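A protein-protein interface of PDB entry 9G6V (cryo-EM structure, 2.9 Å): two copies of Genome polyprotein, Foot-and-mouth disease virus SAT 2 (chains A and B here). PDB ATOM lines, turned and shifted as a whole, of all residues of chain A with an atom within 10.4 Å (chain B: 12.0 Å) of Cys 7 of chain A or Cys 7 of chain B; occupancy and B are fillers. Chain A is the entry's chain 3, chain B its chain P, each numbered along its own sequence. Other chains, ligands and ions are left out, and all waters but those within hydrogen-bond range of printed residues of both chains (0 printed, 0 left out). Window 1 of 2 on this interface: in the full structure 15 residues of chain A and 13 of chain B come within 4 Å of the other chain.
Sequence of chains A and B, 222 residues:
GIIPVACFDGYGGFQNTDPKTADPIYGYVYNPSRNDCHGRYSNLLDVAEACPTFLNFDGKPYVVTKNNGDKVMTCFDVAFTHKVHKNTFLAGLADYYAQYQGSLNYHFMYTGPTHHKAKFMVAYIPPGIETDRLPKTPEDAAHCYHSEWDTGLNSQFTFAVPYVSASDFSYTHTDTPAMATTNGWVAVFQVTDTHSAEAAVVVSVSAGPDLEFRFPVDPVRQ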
ATOM      1  N   ILE A   3       8.126  10.375 -13.360  1.00  0.00           N
ATOM      2  CA  ILE A   3       7.213   9.248 -13.197  1.00  0.00           C
ATOM      3  C   ILE A   3       6.035   9.687 -12.337  1.00  0.00           C
ATOM      4  O   ILE A   3       6.232  10.110 -11.189  1.00  0.00           O
ATOM      5  CB  ILE A   3       7.927   8.040 -12.573  1.00  0.00           C
ATOM      6  CG1 ILE A   3       9.060   7.565 -13.482  1.00  0.00           C
ATOM      7  CG2 ILE A   3       6.942   6.918 -12.311  1.00  0.00           C
ATOM      8  CD1 ILE A   3       9.846   6.404 -12.919  1.00  0.00           C
ATOM      9  N   PRO A   4       4.803   9.612 -12.838  1.00  0.00           N
ATOM     10  CA  PRO A   4       3.648  10.006 -12.022  1.00  0.00           C
ATOM     11  C   PRO A   4       3.276   8.905 -11.036  1.00  0.00           C
ATOM     12  O   PRO A   4       3.077   7.751 -11.420  1.00  0.00           O
ATOM     13  CB  PRO A   4       2.542  10.227 -13.058  1.00  0.00           C
ATOM     14  CG  PRO A   4       2.912   9.321 -14.178  1.00  0.00           C
ATOM     15  CD  PRO A   4       4.416   9.280 -14.219  1.00  0.00           C
ATOM     16  N   VAL A   5       3.189   9.270  -9.759  1.00  0.00           N
ATOM     17  CA  VAL A   5       2.817   8.325  -8.713  1.00  0.00           C
ATOM     18  C   VAL A   5       1.627   8.880  -7.944  1.00  0.00           C
ATOM     19  O   VAL A   5       1.118   9.961  -8.259  1.00  0.00           O
ATOM     20  CB  VAL A   5       3.994   8.034  -7.765  1.00  0.00           C
ATOM     21  CG1 VAL A   5       5.175   7.478  -8.538  1.00  0.00           C
ATOM     22  CG2 VAL A   5       4.388   9.284  -7.001  1.00  0.00           C
ATOM     23  N   ALA A   6       1.173   8.142  -6.934  1.00  0.00           N
ATOM     24  CA  ALA A   6       0.042   8.568  -6.116  1.00  0.00           C
ATOM     25  C   ALA A   6       0.184   7.924  -4.747  1.00  0.00           C
ATOM     26  O   ALA A   6       0.052   6.704  -4.621  1.00  0.00           O
ATOM     27  CB  ALA A   6      -1.281   8.185  -6.768  1.00  0.00           C
ATOM     28  N   CYS A   7       0.448   8.736  -3.728  1.00  0.00           N
ATOM     29  CA  CYS A   7       0.652   8.231  -2.375  1.00  0.00           C
ATOM     30  C   CYS A   7      -0.695   7.821  -1.794  1.00  0.00           C
ATOM     31  O   CYS A   7      -1.513   8.675  -1.439  1.00  0.00           O
ATOM     32  CB  CYS A   7       1.332   9.289  -1.511  1.00  0.00           C
ATOM     33  SG  CYS A   7       1.816   8.725   0.135  1.00  0.00           S
ATOM     34  N   PHE A   8      -0.926   6.515  -1.691  1.00  0.00           N
ATOM     35  CA  PHE A   8      -2.197   6.016  -1.193  1.00  0.00           C
ATOM     36  C   PHE A   8      -2.339   6.267   0.305  1.00  0.00           C
ATOM     37  O   PHE A   8      -1.359   6.406   1.039  1.00  0.00           O
ATOM     38  CB  PHE A   8      -2.339   4.522  -1.481  1.00  0.00           C
ATOM     39  CG  PHE A   8      -2.884   4.219  -2.843  1.00  0.00           C
ATOM     40  CD1 PHE A   8      -3.250   5.241  -3.697  1.00  0.00           C
ATOM     41  CD2 PHE A   8      -3.044   2.915  -3.266  1.00  0.00           C
ATOM     42  CE1 PHE A   8      -3.757   4.971  -4.948  1.00  0.00           C
ATOM     43  CE2 PHE A   8      -3.551   2.638  -4.517  1.00  0.00           C
ATOM     44  CZ  PHE A   8      -3.907   3.668  -5.359  1.00  0.00           C
ATOM     45  N   ASP A   9      -3.590   6.327   0.751  1.00  0.00           N
ATOM     46  CA  ASP A   9      -3.902   6.464   2.166  1.00  0.00           C
ATOM     47  C   ASP A   9      -4.163   5.094   2.771  1.00  0.00           C
ATOM     48  O   ASP A   9      -4.893   4.278   2.202  1.00  0.00           O
ATOM     49  CB  ASP A   9      -5.120   7.365   2.370  1.00  0.00           C
ATOM     50  CG  ASP A   9      -4.886   8.778   1.883  1.00  0.00           C
ATOM     51  OD1 ASP A   9      -3.714   9.208   1.849  1.00  0.00           O
ATOM     52  OD2 ASP A   9      -5.873   9.461   1.536  1.00  0.00           O
ATOM     53  N   GLY A  10      -3.560   4.846   3.929  1.00  0.00           N
ATOM     54  CA  GLY A  10      -3.699   3.565   4.589  1.00  0.00           C
ATOM     55  C   GLY A  10      -2.380   2.841   4.722  1.00  0.00           C
ATOM     56  O   GLY A  10      -2.102   2.220   5.751  1.00  0.00           O
ATOM     57  N   TYR A  11      -1.559   2.916   3.683  1.00  0.00           N
ATOM     58  CA  TYR A  11      -0.227   2.337   3.711  1.00  0.00           C
ATOM     59  C   TYR A  11       0.783   3.384   4.158  1.00  0.00           C
ATOM     60  O   TYR A  11       0.557   4.589   4.025  1.00  0.00           O
ATOM     61  CB  TYR A  11       0.163   1.802   2.335  1.00  0.00           C
ATOM     62  CG  TYR A  11      -0.942   1.066   1.618  1.00  0.00           C
ATOM     63  CD1 TYR A  11      -1.161  -0.284   1.841  1.00  0.00           C
ATOM     64  CD2 TYR A  11      -1.761   1.721   0.711  1.00  0.00           C
ATOM     65  CE1 TYR A  11      -2.166  -0.959   1.184  1.00  0.00           C
ATOM     66  CE2 TYR A  11      -2.768   1.055   0.050  1.00  0.00           C
ATOM     67  CZ  TYR A  11      -2.966  -0.284   0.290  1.00  0.00           C
ATOM     68  OH  TYR A  11      -3.971  -0.950  -0.368  1.00  0.00           O
ATOM     69  N   GLY A  12       1.904   2.913   4.692  1.00  0.00           N
ATOM     70  CA  GLY A  12       2.985   3.786   5.099  1.00  0.00           C
ATOM     71  C   GLY A  12       3.169   3.917   6.591  1.00  0.00           C
ATOM     72  O   GLY A  12       4.218   4.412   7.023  1.00  0.00           O
ATOM     73  N   GLY A  13       2.197   3.497   7.392  1.00  0.00           N
ATOM     74  CA  GLY A  13       2.364   3.552   8.825  1.00  0.00           C
ATOM     75  C   GLY A  13       3.406   2.568   9.314  1.00  0.00           C
ATOM     76  O   GLY A  13       3.764   1.601   8.642  1.00  0.00           O
ATOM     77  N   PHE A  14       3.908   2.827  10.516  1.00  0.00           N
ATOM     78  CA  PHE A  14       4.927   1.968  11.105  1.00  0.00           C
ATOM     79  C   PHE A  14       4.296   0.651  11.537  1.00  0.00           C
ATOM     80  O   PHE A  14       3.482   0.615  12.463  1.00  0.00           O
ATOM     81  CB  PHE A  14       5.592   2.668  12.285  1.00  0.00           C
ATOM     82  CG  PHE A  14       6.499   1.778  13.078  1.00  0.00           C
ATOM     83  CD1 PHE A  14       7.713   1.368  12.559  1.00  0.00           C
ATOM     84  CD2 PHE A  14       6.138   1.352  14.342  1.00  0.00           C
ATOM     85  CE1 PHE A  14       8.547   0.549  13.284  1.00  0.00           C
ATOM     86  CE2 PHE A  14       6.971   0.531  15.072  1.00  0.00           C
ATOM     87  CZ  PHE A  14       8.176   0.131  14.543  1.00  0.00           C
ATOM     88  N   GLN A  15       4.665  -0.432  10.865  1.00  0.00           N
ATOM     89  CA  GLN A  15       4.214  -1.769  11.218  1.00  0.00           C
ATOM     90  C   GLN A  15       5.358  -2.517  11.885  1.00  0.00           C
ATOM     91  O   GLN A  15       6.483  -2.519  11.376  1.00  0.00           O
ATOM     92  CB  GLN A  15       3.741  -2.531   9.981  1.00  0.00           C
ATOM     93  CG  GLN A  15       2.895  -1.708   9.035  1.00  0.00           C
ATOM     94  CD  GLN A  15       2.530  -2.475   7.787  1.00  0.00           C
ATOM     95  OE1 GLN A  15       2.568  -3.705   7.769  1.00  0.00           O
ATOM     96  NE2 GLN A  15       2.176  -1.753   6.730  1.00  0.00           N
ATOM     97  N   LYS A  20       9.538  -5.105   4.997  1.00  0.00           N
ATOM     98  CA  LYS A  20      10.503  -4.181   4.419  1.00  0.00           C
ATOM     99  C   LYS A  20      11.689  -3.979   5.353  1.00  0.00           C
ATOM    100  O   LYS A  20      11.535  -3.908   6.575  1.00  0.00           O
ATOM    101  CB  LYS A  20       9.835  -2.839   4.124  1.00  0.00           C
ATOM    102  CG  LYS A  20       8.480  -2.956   3.445  1.00  0.00           C
ATOM    103  CD  LYS A  20       8.569  -3.741   2.147  1.00  0.00           C
ATOM    104  CE  LYS A  20       7.194  -3.938   1.530  1.00  0.00           C
ATOM    105  NZ  LYS A  20       7.249  -4.776   0.301  1.00  0.00           N
ATOM    106  N   GLY B   1      -2.925   4.644 -15.316  1.00  0.00           N
ATOM    107  CA  GLY B   1      -1.653   5.108 -15.834  1.00  0.00           C
ATOM    108  C   GLY B   1      -0.768   5.716 -14.765  1.00  0.00           C
ATOM    109  O   GLY B   1       0.298   6.256 -15.060  1.00  0.00           O
ATOM    110  N   ILE B   2      -1.215   5.621 -13.516  1.00  0.00           N
ATOM    111  CA  ILE B   2      -0.500   6.166 -12.368  1.00  0.00           C
ATOM    112  C   ILE B   2      -0.019   5.006 -11.510  1.00  0.00           C
ATOM    113  O   ILE B   2      -0.814   4.140 -11.124  1.00  0.00           O
ATOM    114  CB  ILE B   2      -1.392   7.116 -11.552  1.00  0.00           C
ATOM    115  CG1 ILE B   2      -1.951   8.221 -12.447  1.00  0.00           C
ATOM    116  CG2 ILE B   2      -0.613   7.718 -10.405  1.00  0.00           C
ATOM    117  CD1 ILE B   2      -0.891   9.083 -13.078  1.00  0.00           C
ATOM    118  N   ILE B   3       1.276   4.988 -11.215  1.00  0.00           N
ATOM    119  CA  ILE B   3       1.869   3.944 -10.384  1.00  0.00           C
ATOM    120  C   ILE B   3       1.499   4.197  -8.927  1.00  0.00           C
ATOM    121  O   ILE B   3       1.829   5.259  -8.384  1.00  0.00           O
ATOM    122  CB  ILE B   3       3.394   3.891 -10.561  1.00  0.00           C
ATOM    123  CG1 ILE B   3       3.748   3.560 -12.011  1.00  0.00           C
ATOM    124  CG2 ILE B   3       4.002   2.875  -9.616  1.00  0.00           C
ATOM    125  CD1 ILE B   3       5.233   3.542 -12.286  1.00  0.00           C
ATOM    126  N   PRO B   4       0.823   3.264  -8.259  1.00  0.00           N
ATOM    127  CA  PRO B   4       0.489   3.466  -6.843  1.00  0.00           C
ATOM    128  C   PRO B   4       1.703   3.220  -5.960  1.00  0.00           C
ATOM    129  O   PRO B   4       2.369   2.188  -6.069  1.00  0.00           O
ATOM    130  CB  PRO B   4      -0.610   2.432  -6.587  1.00  0.00           C
ATOM    131  CG  PRO B   4      -0.326   1.352  -7.571  1.00  0.00           C
ATOM    132  CD  PRO B   4       0.232   2.026  -8.795  1.00  0.00           C
ATOM    133  N   VAL B   5       1.992   4.178  -5.081  1.00  0.00           N
ATOM    134  CA  VAL B   5       3.106   4.097  -4.154  1.00  0.00           C
ATOM    135  C   VAL B   5       2.587   4.373  -2.748  1.00  0.00           C
ATOM    136  O   VAL B   5       1.395   4.581  -2.533  1.00  0.00           O
ATOM    137  CB  VAL B   5       4.248   5.068  -4.517  1.00  0.00           C
ATOM    138  CG1 VAL B   5       4.761   4.786  -5.915  1.00  0.00           C
ATOM    139  CG2 VAL B   5       3.782   6.505  -4.391  1.00  0.00           C
ATOM    140  N   ALA B   6       3.506   4.366  -1.783  1.00  0.00           N
ATOM    141  CA  ALA B   6       3.149   4.615  -0.391  1.00  0.00           C
ATOM    142  C   ALA B   6       4.386   5.139   0.323  1.00  0.00           C
ATOM    143  O   ALA B   6       5.355   4.396   0.501  1.00  0.00           O
ATOM    144  CB  ALA B   6       2.628   3.349   0.270  1.00  0.00           C
ATOM    145  N   CYS B   7       4.351   6.403   0.733  1.00  0.00           N
ATOM    146  CA  CYS B   7       5.495   7.035   1.387  1.00  0.00           C
ATOM    147  C   CYS B   7       5.584   6.514   2.815  1.00  0.00           C
ATOM    148  O   CYS B   7       4.824   6.931   3.690  1.00  0.00           O
ATOM    149  CB  CYS B   7       5.357   8.552   1.352  1.00  0.00           C
ATOM    150  SG  CYS B   7       6.778   9.453   2.012  1.00  0.00           S
ATOM    151  N   PHE B   8       6.518   5.599   3.054  1.00  0.00           N
ATOM    152  CA  PHE B   8       6.660   4.997   4.371  1.00  0.00           C
ATOM    153  C   PHE B   8       7.184   6.005   5.386  1.00  0.00           C
ATOM    154  O   PHE B   8       7.965   6.903   5.062  1.00  0.00           O
ATOM    155  CB  PHE B   8       7.596   3.791   4.314  1.00  0.00           C
ATOM    156  CG  PHE B   8       6.895   2.495   4.033  1.00  0.00           C
ATOM    157  CD1 PHE B   8       5.663   2.482   3.409  1.00  0.00           C
ATOM    158  CD2 PHE B   8       7.461   1.294   4.412  1.00  0.00           C
ATOM    159  CE1 PHE B   8       5.012   1.294   3.156  1.00  0.00           C
ATOM    160  CE2 PHE B   8       6.815   0.102   4.162  1.00  0.00           C
ATOM    161  CZ  PHE B   8       5.589   0.103   3.533  1.00  0.00           C
ATOM    162  N   ASP B   9       6.740   5.846   6.629  1.00  0.00           N
ATOM    163  CA  ASP B   9       7.225   6.659   7.735  1.00  0.00           C
ATOM    164  C   ASP B   9       8.479   6.032   8.323  1.00  0.00           C
ATOM    165  O   ASP B   9       8.539   4.819   8.541  1.00  0.00           O
ATOM    166  CB  ASP B   9       6.156   6.800   8.819  1.00  0.00           C
ATOM    167  CG  ASP B   9       4.916   7.512   8.324  1.00  0.00           C
ATOM    168  OD1 ASP B   9       5.029   8.307   7.368  1.00  0.00           O
ATOM    169  OD2 ASP B   9       3.828   7.278   8.893  1.00  0.00           O
ATOM    170  N   GLY B  10       9.480   6.867   8.580  1.00  0.00           N
ATOM    171  CA  GLY B  10      10.740   6.394   9.114  1.00  0.00           C
ATOM    172  C   GLY B  10      11.889   6.624   8.161  1.00  0.00           C
ATOM    173  O   GLY B  10      12.982   7.019   8.574  1.00  0.00           O
ATOM    174  N   TYR B  11      11.654   6.382   6.878  1.00  0.00           N
ATOM    175  CA  TYR B  11      12.640   6.666   5.852  1.00  0.00           C
ATOM    176  C   TYR B  11      12.410   8.063   5.293  1.00  0.00           C
ATOM    177  O   TYR B  11      11.283   8.561   5.262  1.00  0.00           O
ATOM    178  CB  TYR B  11      12.564   5.641   4.723  1.00  0.00           C
ATOM    179  CG  TYR B  11      12.367   4.218   5.183  1.00  0.00           C
ATOM    180  CD1 TYR B  11      13.449   3.423   5.527  1.00  0.00           C
ATOM    181  CD2 TYR B  11      11.097   3.666   5.262  1.00  0.00           C
ATOM    182  CE1 TYR B  11      13.271   2.121   5.943  1.00  0.00           C
ATOM    183  CE2 TYR B  11      10.911   2.367   5.677  1.00  0.00           C
ATOM    184  CZ  TYR B  11      12.000   1.600   6.015  1.00  0.00           C
ATOM    185  OH  TYR B  11      11.815   0.302   6.429  1.00  0.00           O
ATOM    186  N   GLY B  12      13.492   8.693   4.850  1.00  0.00           N
ATOM    187  CA  GLY B  12      13.436  10.007   4.238  1.00  0.00           C
ATOM    188  C   GLY B  12      14.237  11.070   4.954  1.00  0.00           C
ATOM    189  O   GLY B  12      14.464  12.145   4.382  1.00  0.00           O
ATOM    190  N   GLY B  13      14.674  10.816   6.181  1.00  0.00           N
ATOM    191  CA  GLY B  13      15.456  11.799   6.894  1.00  0.00           C
ATOM    192  C   GLY B  13      16.831  11.985   6.288  1.00  0.00           C
ATOM    193  O   GLY B  13      17.318  11.176   5.499  1.00  0.00           O
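The side-chain sulfur (SG) of Cys 7 of chain A is in hydrogen-bond range of the backbone NH (N) of Cys 7 of chain B. N of Ile 3 of chain B sits at hydrogen-bond distance from O of Pro 4 of chain A (3.3 Å). The backbone NH (N) of Asp 9 of chain B sits at hydrogen-bond distance from the backbone carbonyl oxygen (O) of Gly 12 of chain A, 2.9 Å away. O of Val 5 of chain B sits at hydrogen-bond distance from N of Phe 8 of chain A. N of Ala 6 of chain A sits at hydrogen-bond distance from O of Ile 3 of chain B, 3.3 Å away. O of Ala 6 of chain A is in hydrogen-bond range of N of Val 5 of chain B (3.2 Å).
Among the printed residues, pairs that only touch across the chains: Ile 3 of chain A with Ile 3 of chain B, Pro 4 of chain A with Ile 2 of chain B, Val 5 of chain A with Ile 2 of chain B, Val 5 of chain A with Ile 3 of chain B, Val 5 of chain A with Val 5 of chain B, Ala 6 of chain A with Ile 2 of chain B, Ala 6 of chain A with Pro 4 of chain B, Cys 7 of chain A with Val 5 of chain B, Phe 8 of chain A with Pro 4 of chain B, Tyr 11 of chain A with Ala 6 of chain B, Gly 12 of chain A with Cys 7 of chain B, Gly 12 of chain A with Phe 8 of chain B and Lys 20 of chain A with Phe 8 of chain B.
Of chain B, only Ile 2 (3.5 Å), Ile 3 (3.2 Å) and Val 5 (3.7 Å) come within 4 Å of Val 5 of chain A. Ala 6 of chain A touches four residues of chain B. Cys 7 of chain A touches just these residues of chain B: Val 5 (3.7 Å) and Cys 7 (3.5 Å). Phe 8 of chain A touches two residues of chain B. No residue of chain B comes within 4 Å of Asp 9 of chain A. Gly 1 of chain B touches none of the printed residues of chain A. Of the printed residues of chain A, Ile 2 of chain B touches Pro 4, Val 5 and Ala 6. Printed residues of chain A within 4 Å of Ile 3 of chain B: Ile 3, Pro 4, Val 5 and Ala 6. Of the printed residues of chain A, Pro 4 of chain B touches Ala 6 (3.95 Å) and Phe 8 (3.6 Å). Of chain A, only Val 5 (3.7 Å), Ala 6 (3.2 Å), Cys 7 (3.7 Å) and Phe 8 (3.1 Å) come within 4 Å of Val 5 of chain B. Ala 6 of chain B touches just one residue of chain A: Tyr 11 (3.6 Å). Cys 7 of chain B touches just these residues of chain A: Cys 7 (3.5 Å) and Gly 12 (3.9 Å). Printed residues of chain A within 4 Å of Phe 8 of chain B: Gly 12 (3.4 Å) and Lys 20 (3.6 Å). Tyr 11 of chain B touches none of the printed residues of chain A. The nearest residue of chain B that does not touch Cys 7 of chain A is Ala 6 of chain B (4.4 Å). The nearest residue of chain A that does not touch Cys 7 of chain B is Tyr 11 of chain A (4.9 Å).
Of the 13 printed residues of chain B, 8 touch a printed residue of chain A. Printed residues of chain B that touch a printed residue of chain A: Ile 2, Ile 3, Pro 4, Val 5, Ala 6, Cys 7, Phe 8 and Asp 9. Hydrophobic or aromatic side chains of chain B that line the printed part of chain A: Ile 2, Ile 3, Pro 4, Val 5, Ala 6 and Phe 8. Among the printed residues, 19 pairs touch across the chains. Among the printed residues, no Asp or Glu carboxylate lies within 4 Å of a Lys or Arg side-chain nitrogen of the other chain.
Ile 3 of chain B touches its own counterpart, Ile 3 of chain A. Pro 4 of chain A touches Ile 3 of chain B, but with the chains exchanged Ile 3 of chain A does not touch Pro 4 of chain B (8.2 Å). Ala 6 of chain A touches Pro 4 of chain B, but with the chains exchanged Pro 4 of chain A does not touch Ala 6 of chain B (10.2 Å). Phe 8 of chain A touches Pro 4 of chain B, but with the chains exchanged Pro 4 of chain A does not touch Phe 8 of chain B (14.8 Å). Of the 19 pairs that touch across the chains among the printed residues, 3 have their exchanged pair printed and touching as well.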
